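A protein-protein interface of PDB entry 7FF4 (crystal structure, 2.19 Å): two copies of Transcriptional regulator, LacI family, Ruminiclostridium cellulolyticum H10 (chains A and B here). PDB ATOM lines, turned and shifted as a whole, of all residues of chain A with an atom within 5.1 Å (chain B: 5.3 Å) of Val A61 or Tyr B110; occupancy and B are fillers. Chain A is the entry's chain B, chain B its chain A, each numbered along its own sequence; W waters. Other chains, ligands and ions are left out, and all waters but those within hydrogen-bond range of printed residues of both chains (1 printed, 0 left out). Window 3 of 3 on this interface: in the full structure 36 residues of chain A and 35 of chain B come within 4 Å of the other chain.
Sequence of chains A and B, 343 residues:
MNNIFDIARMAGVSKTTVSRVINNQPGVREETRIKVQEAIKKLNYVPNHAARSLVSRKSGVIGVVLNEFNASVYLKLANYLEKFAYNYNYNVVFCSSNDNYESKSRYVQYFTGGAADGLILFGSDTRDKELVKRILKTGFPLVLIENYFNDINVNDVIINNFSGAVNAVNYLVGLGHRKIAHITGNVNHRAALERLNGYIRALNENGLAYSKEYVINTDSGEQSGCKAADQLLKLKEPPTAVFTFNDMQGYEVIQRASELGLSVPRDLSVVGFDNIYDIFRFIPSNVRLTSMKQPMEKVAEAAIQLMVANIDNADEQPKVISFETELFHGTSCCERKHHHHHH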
ATOM      1  N   GLY A  60      14.089 -16.948 -22.439  1.00  0.00           N
ATOM      2  CA  GLY A  60      12.866 -16.423 -23.072  1.00  0.00           C
ATOM      3  C   GLY A  60      13.007 -14.955 -23.426  1.00  0.00           C
ATOM      4  O   GLY A  60      13.790 -14.279 -22.778  1.00  0.00           O
ATOM      5  N   VAL A  61      12.245 -14.491 -24.410  1.00  0.00           N
ATOM      6  CA  VAL A  61      12.361 -13.074 -24.844  1.00  0.00           C
ATOM      7  C   VAL A  61      10.986 -12.413 -24.928  1.00  0.00           C
ATOM      8  O   VAL A  61      10.104 -12.961 -25.577  1.00  0.00           O
ATOM      9  CB  VAL A  61      13.092 -12.972 -26.193  1.00  0.00           C
ATOM     10  CG1 VAL A  61      12.878 -11.617 -26.830  1.00  0.00           C
ATOM     11  CG2 VAL A  61      14.572 -13.262 -26.049  1.00  0.00           C
ATOM     12  N   ILE A  62      10.852 -11.265 -24.275  1.00  0.00           N
ATOM     13  CA  ILE A  62       9.617 -10.442 -24.353  1.00  0.00           C
ATOM     14  C   ILE A  62       9.982  -9.218 -25.180  1.00  0.00           C
ATOM     15  O   ILE A  62      10.949  -8.569 -24.846  1.00  0.00           O
ATOM     16  CB  ILE A  62       9.123 -10.038 -22.958  1.00  0.00           C
ATOM     17  CG1 ILE A  62       8.593 -11.232 -22.170  1.00  0.00           C
ATOM     18  CG2 ILE A  62       8.074  -8.955 -23.080  1.00  0.00           C
ATOM     19  CD1 ILE A  62       8.523 -10.997 -20.698  1.00  0.00           C
ATOM     20  N   GLY A  63       9.219  -8.939 -26.223  1.00  0.00           N
ATOM     21  CA  GLY A  63       9.507  -7.794 -27.094  1.00  0.00           C
ATOM     22  C   GLY A  63       8.615  -6.613 -26.788  1.00  0.00           C
ATOM     23  O   GLY A  63       7.462  -6.822 -26.454  1.00  0.00           O
ATOM     24  N   TYR A  90      13.561 -13.720 -17.904  1.00  0.00           N
ATOM     25  CA  TYR A  90      13.180 -13.366 -19.291  1.00  0.00           C
ATOM     26  C   TYR A  90      14.043 -12.200 -19.764  1.00  0.00           C
ATOM     27  O   TYR A  90      14.462 -11.402 -18.948  1.00  0.00           O
ATOM     28  CB  TYR A  90      11.711 -12.966 -19.353  1.00  0.00           C
ATOM     29  CG  TYR A  90      10.775 -14.098 -19.655  1.00  0.00           C
ATOM     30  CD1 TYR A  90      10.376 -14.968 -18.666  1.00  0.00           C
ATOM     31  CD2 TYR A  90      10.293 -14.299 -20.928  1.00  0.00           C
ATOM     32  CE1 TYR A  90       9.519 -16.015 -18.929  1.00  0.00           C
ATOM     33  CE2 TYR A  90       9.441 -15.347 -21.214  1.00  0.00           C
ATOM     34  CZ  TYR A  90       9.054 -16.208 -20.210  1.00  0.00           C
ATOM     35  OH  TYR A  90       8.214 -17.241 -20.478  1.00  0.00           O
ATOM     36  N   ASN A  91      14.319 -12.151 -21.059  1.00  0.00           N
ATOM     37  CA  ASN A  91      15.072 -11.009 -21.624  1.00  0.00           C
ATOM     38  C   ASN A  91      14.044 -10.042 -22.196  1.00  0.00           C
ATOM     39  O   ASN A  91      13.023 -10.515 -22.662  1.00  0.00           O
ATOM     40  CB  ASN A  91      15.992 -11.440 -22.758  1.00  0.00           C
ATOM     41  CG  ASN A  91      17.248 -12.133 -22.295  1.00  0.00           C
ATOM     42  OD1 ASN A  91      17.697 -11.954 -21.178  1.00  0.00           O
ATOM     43  ND2 ASN A  91      17.832 -12.923 -23.164  1.00  0.00           N
ATOM     44  N   VAL A  93      13.442  -6.894 -24.982  1.00  0.00           N
ATOM     45  CA  VAL A  93      14.074  -6.232 -26.149  1.00  0.00           C
ATOM     46  C   VAL A  93      13.142  -5.132 -26.647  1.00  0.00           C
ATOM     47  O   VAL A  93      11.961  -5.388 -26.797  1.00  0.00           O
ATOM     48  CB  VAL A  93      14.381  -7.277 -27.227  1.00  0.00           C
ATOM     49  CG1 VAL A  93      14.488  -6.662 -28.601  1.00  0.00           C
ATOM     50  CG2 VAL A  93      15.634  -8.047 -26.883  1.00  0.00           C
ATOM     51  N   TYR A 110       8.459  -8.896 -36.690  1.00  0.00           N
ATOM     52  CA  TYR A 110       9.764  -9.465 -36.297  1.00  0.00           C
ATOM     53  C   TYR A 110       9.556 -10.253 -35.011  1.00  0.00           C
ATOM     54  O   TYR A 110      10.078 -11.354 -34.894  1.00  0.00           O
ATOM     55  CB  TYR A 110      10.809  -8.355 -36.170  1.00  0.00           C
ATOM     56  CG  TYR A 110      12.039  -8.695 -35.374  1.00  0.00           C
ATOM     57  CD1 TYR A 110      13.075  -9.410 -35.930  1.00  0.00           C
ATOM     58  CD2 TYR A 110      12.167  -8.294 -34.063  1.00  0.00           C
ATOM     59  CE1 TYR A 110      14.205  -9.724 -35.205  1.00  0.00           C
ATOM     60  CE2 TYR A 110      13.290  -8.593 -33.322  1.00  0.00           C
ATOM     61  CZ  TYR A 110      14.311  -9.315 -33.894  1.00  0.00           C
ATOM     62  OH  TYR A 110      15.414  -9.618 -33.165  1.00  0.00           O
ATOM     63  N   ALA A 115      11.185 -13.966 -32.968  1.00  0.00           N
ATOM     64  CA  ALA A 115      12.257 -13.326 -32.179  1.00  0.00           C
ATOM     65  C   ALA A 115      11.830 -13.218 -30.717  1.00  0.00           C
ATOM     66  O   ALA A 115      12.699 -13.156 -29.868  1.00  0.00           O
ATOM     67  CB  ALA A 115      12.612 -11.986 -32.754  1.00  0.00           C
ATOM     68  N   ALA A 116      10.533 -13.239 -30.441  1.00  0.00           N
ATOM     69  CA  ALA A 116      10.103 -13.137 -29.033  1.00  0.00           C
ATOM     70  C   ALA A 116       8.937 -14.073 -28.734  1.00  0.00           C
ATOM     71  O   ALA A 116       8.271 -14.509 -29.651  1.00  0.00           O
ATOM     72  CB  ALA A 116       9.718 -11.721 -28.733  1.00  0.00           C
ATOM     73  N   ASP A 117       8.711 -14.324 -27.455  1.00  0.00           N
ATOM     74  CA  ASP A 117       7.599 -15.183 -27.002  1.00  0.00           C
ATOM     75  C   ASP A 117       6.378 -14.304 -26.726  1.00  0.00           C
ATOM     76  O   ASP A 117       5.275 -14.816 -26.799  1.00  0.00           O
ATOM     77  CB  ASP A 117       8.048 -16.007 -25.804  1.00  0.00           C
ATOM     78  CG  ASP A 117       9.291 -16.800 -26.135  1.00  0.00           C
ATOM     79  OD1 ASP A 117       9.328 -17.355 -27.222  1.00  0.00           O
ATOM     80  OD2 ASP A 117      10.205 -16.831 -25.322  1.00  0.00           O
ATOM     81  N   GLY A 118       6.582 -13.011 -26.474  1.00  0.00           N
ATOM     82  CA  GLY A 118       5.453 -12.110 -26.184  1.00  0.00           C
ATOM     83  C   GLY A 118       5.707 -10.687 -26.629  1.00  0.00           C
ATOM     84  O   GLY A 118       6.852 -10.326 -26.792  1.00  0.00           O
ATOM     85  N   CYS B  95      18.403  -2.947 -25.663  1.00  0.00           N
ATOM     86  CA  CYS B  95      18.317  -3.634 -24.360  1.00  0.00           C
ATOM     87  C   CYS B  95      18.853  -2.715 -23.276  1.00  0.00           C
ATOM     88  O   CYS B  95      19.809  -2.025 -23.540  1.00  0.00           O
ATOM     89  CB  CYS B  95      19.211  -4.855 -24.358  1.00  0.00           C
ATOM     90  SG  CYS B  95      18.433  -6.233 -25.214  1.00  0.00           S
ATOM     91  N   SER B 105      26.282  -8.170 -19.552  1.00  0.00           N
ATOM     92  CA  SER B 105      26.994  -9.360 -20.083  1.00  0.00           C
ATOM     93  C   SER B 105      25.979 -10.306 -20.706  1.00  0.00           C
ATOM     94  O   SER B 105      26.224 -10.816 -21.775  1.00  0.00           O
ATOM     95  CB  SER B 105      27.742 -10.055 -19.000  1.00  0.00           C
ATOM     96  OG  SER B 105      29.095  -9.661 -18.991  1.00  0.00           O
ATOM     97  N   ARG B 106      24.868 -10.497 -20.022  1.00  0.00           N
ATOM     98  CA  ARG B 106      23.810 -11.391 -20.524  1.00  0.00           C
ATOM     99  C   ARG B 106      23.328 -10.895 -21.884  1.00  0.00           C
ATOM    100  O   ARG B 106      23.201 -11.703 -22.785  1.00  0.00           O
ATOM    101  CB  ARG B 106      22.673 -11.400 -19.508  1.00  0.00           C
ATOM    102  CG  ARG B 106      21.442 -12.159 -19.962  1.00  0.00           C
ATOM    103  CD  ARG B 106      20.520 -12.340 -18.783  1.00  0.00           C
ATOM    104  NE  ARG B 106      20.233 -11.077 -18.125  1.00  0.00           N
ATOM    105  CZ  ARG B 106      19.192 -10.322 -18.420  1.00  0.00           C
ATOM    106  NH1 ARG B 106      18.365 -10.704 -19.372  1.00  0.00           N
ATOM    107  NH2 ARG B 106      18.987  -9.193 -17.777  1.00  0.00           N
ATOM    108  N   TYR B 107      23.045  -9.600 -21.996  1.00  0.00           N
ATOM    109  CA  TYR B 107      22.540  -9.042 -23.271  1.00  0.00           C
ATOM    110  C   TYR B 107      23.617  -9.155 -24.343  1.00  0.00           C
ATOM    111  O   TYR B 107      23.289  -9.444 -25.465  1.00  0.00           O
ATOM    112  CB  TYR B 107      21.934  -7.652 -23.073  1.00  0.00           C
ATOM    113  CG  TYR B 107      20.547  -7.709 -22.498  1.00  0.00           C
ATOM    114  CD1 TYR B 107      19.523  -8.283 -23.208  1.00  0.00           C
ATOM    115  CD2 TYR B 107      20.271  -7.243 -21.232  1.00  0.00           C
ATOM    116  CE1 TYR B 107      18.250  -8.372 -22.692  1.00  0.00           C
ATOM    117  CE2 TYR B 107      19.002  -7.321 -20.697  1.00  0.00           C
ATOM    118  CZ  TYR B 107      17.989  -7.891 -21.432  1.00  0.00           C
ATOM    119  OH  TYR B 107      16.733  -7.991 -20.941  1.00  0.00           O
ATOM    120  N   VAL B 108      24.870  -8.933 -23.995  1.00  0.00           N
ATOM    121  CA  VAL B 108      25.927  -9.088 -25.025  1.00  0.00           C
ATOM    122  C   VAL B 108      25.928 -10.539 -25.517  1.00  0.00           C
ATOM    123  O   VAL B 108      25.990 -10.736 -26.716  1.00  0.00           O
ATOM    124  CB  VAL B 108      27.291  -8.668 -24.473  1.00  0.00           C
ATOM    125  CG1 VAL B 108      28.412  -9.028 -25.420  1.00  0.00           C
ATOM    126  CG2 VAL B 108      27.319  -7.195 -24.155  1.00  0.00           C
ATOM    127  N   GLN B 109      25.814 -11.511 -24.610  1.00  0.00           N
ATOM    128  CA  GLN B 109      25.809 -12.944 -24.997  1.00  0.00           C
ATOM    129  C   GLN B 109      24.577 -13.222 -25.851  1.00  0.00           C
ATOM    130  O   GLN B 109      24.683 -13.976 -26.800  1.00  0.00           O
ATOM    131  CB  GLN B 109      25.832 -13.861 -23.771  1.00  0.00           C
ATOM    132  CG  GLN B 109      27.040 -13.657 -22.869  1.00  0.00           C
ATOM    133  CD  GLN B 109      27.191 -14.675 -21.759  1.00  0.00           C
ATOM    134  OE1 GLN B 109      26.302 -14.876 -20.934  1.00  0.00           O
ATOM    135  NE2 GLN B 109      28.349 -15.315 -21.713  1.00  0.00           N
ATOM    136  N   TYR B 110      23.457 -12.592 -25.527  1.00  0.00           N
ATOM    137  CA  TYR B 110      22.228 -12.798 -26.325  1.00  0.00           C
ATOM    138  C   TYR B 110      22.496 -12.388 -27.771  1.00  0.00           C
ATOM    139  O   TYR B 110      22.132 -13.112 -28.675  1.00  0.00           O
ATOM    140  CB  TYR B 110      21.070 -12.009 -25.717  1.00  0.00           C
ATOM    141  CG  TYR B 110      19.828 -11.901 -26.562  1.00  0.00           C
ATOM    142  CD1 TYR B 110      19.015 -12.990 -26.782  1.00  0.00           C
ATOM    143  CD2 TYR B 110      19.451 -10.699 -27.123  1.00  0.00           C
ATOM    144  CE1 TYR B 110      17.870 -12.897 -27.550  1.00  0.00           C
ATOM    145  CE2 TYR B 110      18.310 -10.585 -27.895  1.00  0.00           C
ATOM    146  CZ  TYR B 110      17.510 -11.687 -28.104  1.00  0.00           C
ATOM    147  OH  TYR B 110      16.395 -11.595 -28.873  1.00  0.00           O
ATOM    148  N   PHE B 111      23.111 -11.230 -27.968  1.00  0.00           N
ATOM    149  CA  PHE B 111      23.334 -10.711 -29.338  1.00  0.00           C
ATOM    150  C   PHE B 111      24.429 -11.498 -30.049  1.00  0.00           C
ATOM    151  O   PHE B 111      24.228 -11.871 -31.176  1.00  0.00           O
ATOM    152  CB  PHE B 111      23.618  -9.211 -29.303  1.00  0.00           C
ATOM    153  CG  PHE B 111      22.415  -8.367 -28.996  1.00  0.00           C
ATOM    154  CD1 PHE B 111      21.212  -8.603 -29.621  1.00  0.00           C
ATOM    155  CD2 PHE B 111      22.486  -7.344 -28.080  1.00  0.00           C
ATOM    156  CE1 PHE B 111      20.101  -7.834 -29.335  1.00  0.00           C
ATOM    157  CE2 PHE B 111      21.376  -6.577 -27.792  1.00  0.00           C
ATOM    158  CZ  PHE B 111      20.186  -6.823 -28.420  1.00  0.00           C
ATOM    159  N   THR B 112      25.570 -11.695 -29.402  1.00  0.00           N
ATOM    160  CA  THR B 112      26.684 -12.431 -30.049  1.00  0.00           C
ATOM    161  C   THR B 112      26.289 -13.894 -30.234  1.00  0.00           C
ATOM    162  O   THR B 112      26.875 -14.536 -31.075  1.00  0.00           O
ATOM    163  CB  THR B 112      27.976 -12.297 -29.253  1.00  0.00           C
ATOM    164  OG1 THR B 112      27.717 -12.894 -27.992  1.00  0.00           O
ATOM    165  CG2 THR B 112      28.364 -10.857 -29.038  1.00  0.00           C
ATOM    166  N   GLY B 113      25.293 -14.370 -29.496  1.00  0.00           N
ATOM    167  CA  GLY B 113      24.831 -15.759 -29.611  1.00  0.00           C
ATOM    168  C   GLY B 113      23.933 -15.965 -30.812  1.00  0.00           C
ATOM    169  O   GLY B 113      23.415 -17.064 -30.967  1.00  0.00           O
ATOM    170  N   GLY B 114      23.676 -14.939 -31.611  1.00  0.00           N
ATOM    171  CA  GLY B 114      22.834 -15.207 -32.789  1.00  0.00           C
ATOM    172  C   GLY B 114      21.635 -14.299 -32.919  1.00  0.00           C
ATOM    173  O   GLY B 114      21.030 -14.299 -33.975  1.00  0.00           O
ATOM    174  N   ALA B 115      21.291 -13.545 -31.888  1.00  0.00           N
ATOM    175  CA  ALA B 115      20.115 -12.667 -32.040  1.00  0.00           C
ATOM    176  C   ALA B 115      20.425 -11.493 -32.977  1.00  0.00           C
ATOM    177  O   ALA B 115      19.516 -11.034 -33.630  1.00  0.00           O
ATOM    178  CB  ALA B 115      19.638 -12.208 -30.694  1.00  0.00           C
ATOM    179  N   ALA B 116      21.675 -11.049 -33.056  1.00  0.00           N
ATOM    180  CA  ALA B 116      21.995  -9.911 -33.941  1.00  0.00           C
ATOM    181  C   ALA B 116      23.245 -10.196 -34.766  1.00  0.00           C
ATOM    182  O   ALA B 116      23.973 -11.106 -34.427  1.00  0.00           O
ATOM    183  CB  ALA B 116      22.185  -8.672 -33.122  1.00  0.00           C
HETATM  184  O   HOH W   1      17.020 -11.761 -33.901  1.00  0.00           O
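3 positions are printed for both chains.
Of the 7 pairs that touch across the chains among the printed residues, none has its exchanged pair printed and touching as well.
Among the printed residues, pairs that only touch across the chains: Val A61 with Tyr B110, Tyr A90 with Arg B106, Asn A91 with Tyr B107, Asn A91 with Tyr B110, Val A93 with Cys B95 and Val A93 with Tyr B110.
Of the 13 printed residues of chain B, 4 touch a printed residue of chain A.
Hydrophobic or aromatic side chains of chain B that line the printed part of chain A: Tyr B107 and Tyr B110.
Along chain B the printed residues that touch a printed residue of chain A span positions 95 to 110.
Of the 12 printed residues of chain A, 4 touch a printed residue of chain B.
Printed residues of chain A that touch a printed residue of chain B: Val A61, Tyr A90, Asn A91 and Val A93.
Among the printed residues, 7 pairs touch across the chains.
Val A61 touches just one residue of chain B: Tyr B110 (3.6 Å).
Tyr B110 touches three residues of chain A.
Of the printed residues of chain A, Arg B106 touches Tyr A90 and Asn A91.
Of the printed residues of chain B, Tyr A90 touches Arg B106 (3.99 Å).
Of the printed residues of chain B, Val A93 touches Cys B95 and Tyr B110.
Of the printed residues of chain B, Asn A91 touches Arg B106 (2.3 Å), Tyr B107 (3.5 Å) and Tyr B110 (3.8 Å).
Of the printed residues of chain A, Cys B95 touches Val A93.
The nearest printed residue of chain B that does not touch Val A61 is Ala B115 (7.0 Å).
The side-chain amide oxygen of Asn A91 sits close to the guanidinium group of Arg B106, at 2.3 Å.
O of Ile A62 lies within hydrogen-bond range of N of Val A93 (3.0 Å).
N of Asp A117 is in hydrogen-bond range of O of Val A61, at 2.7 Å.
O of Asn A91 sits at hydrogen-bond distance from N of Ile A62 (2.8 Å).
N of Asn A91 sits at hydrogen-bond distance from O of Gly A60 (2.8 Å).
N of Ala B115 lies close to O of Tyr B110 (3.3 Å).
Water W1 lies within hydrogen-bond range of O of Ala B115 and OH of Tyr A110.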
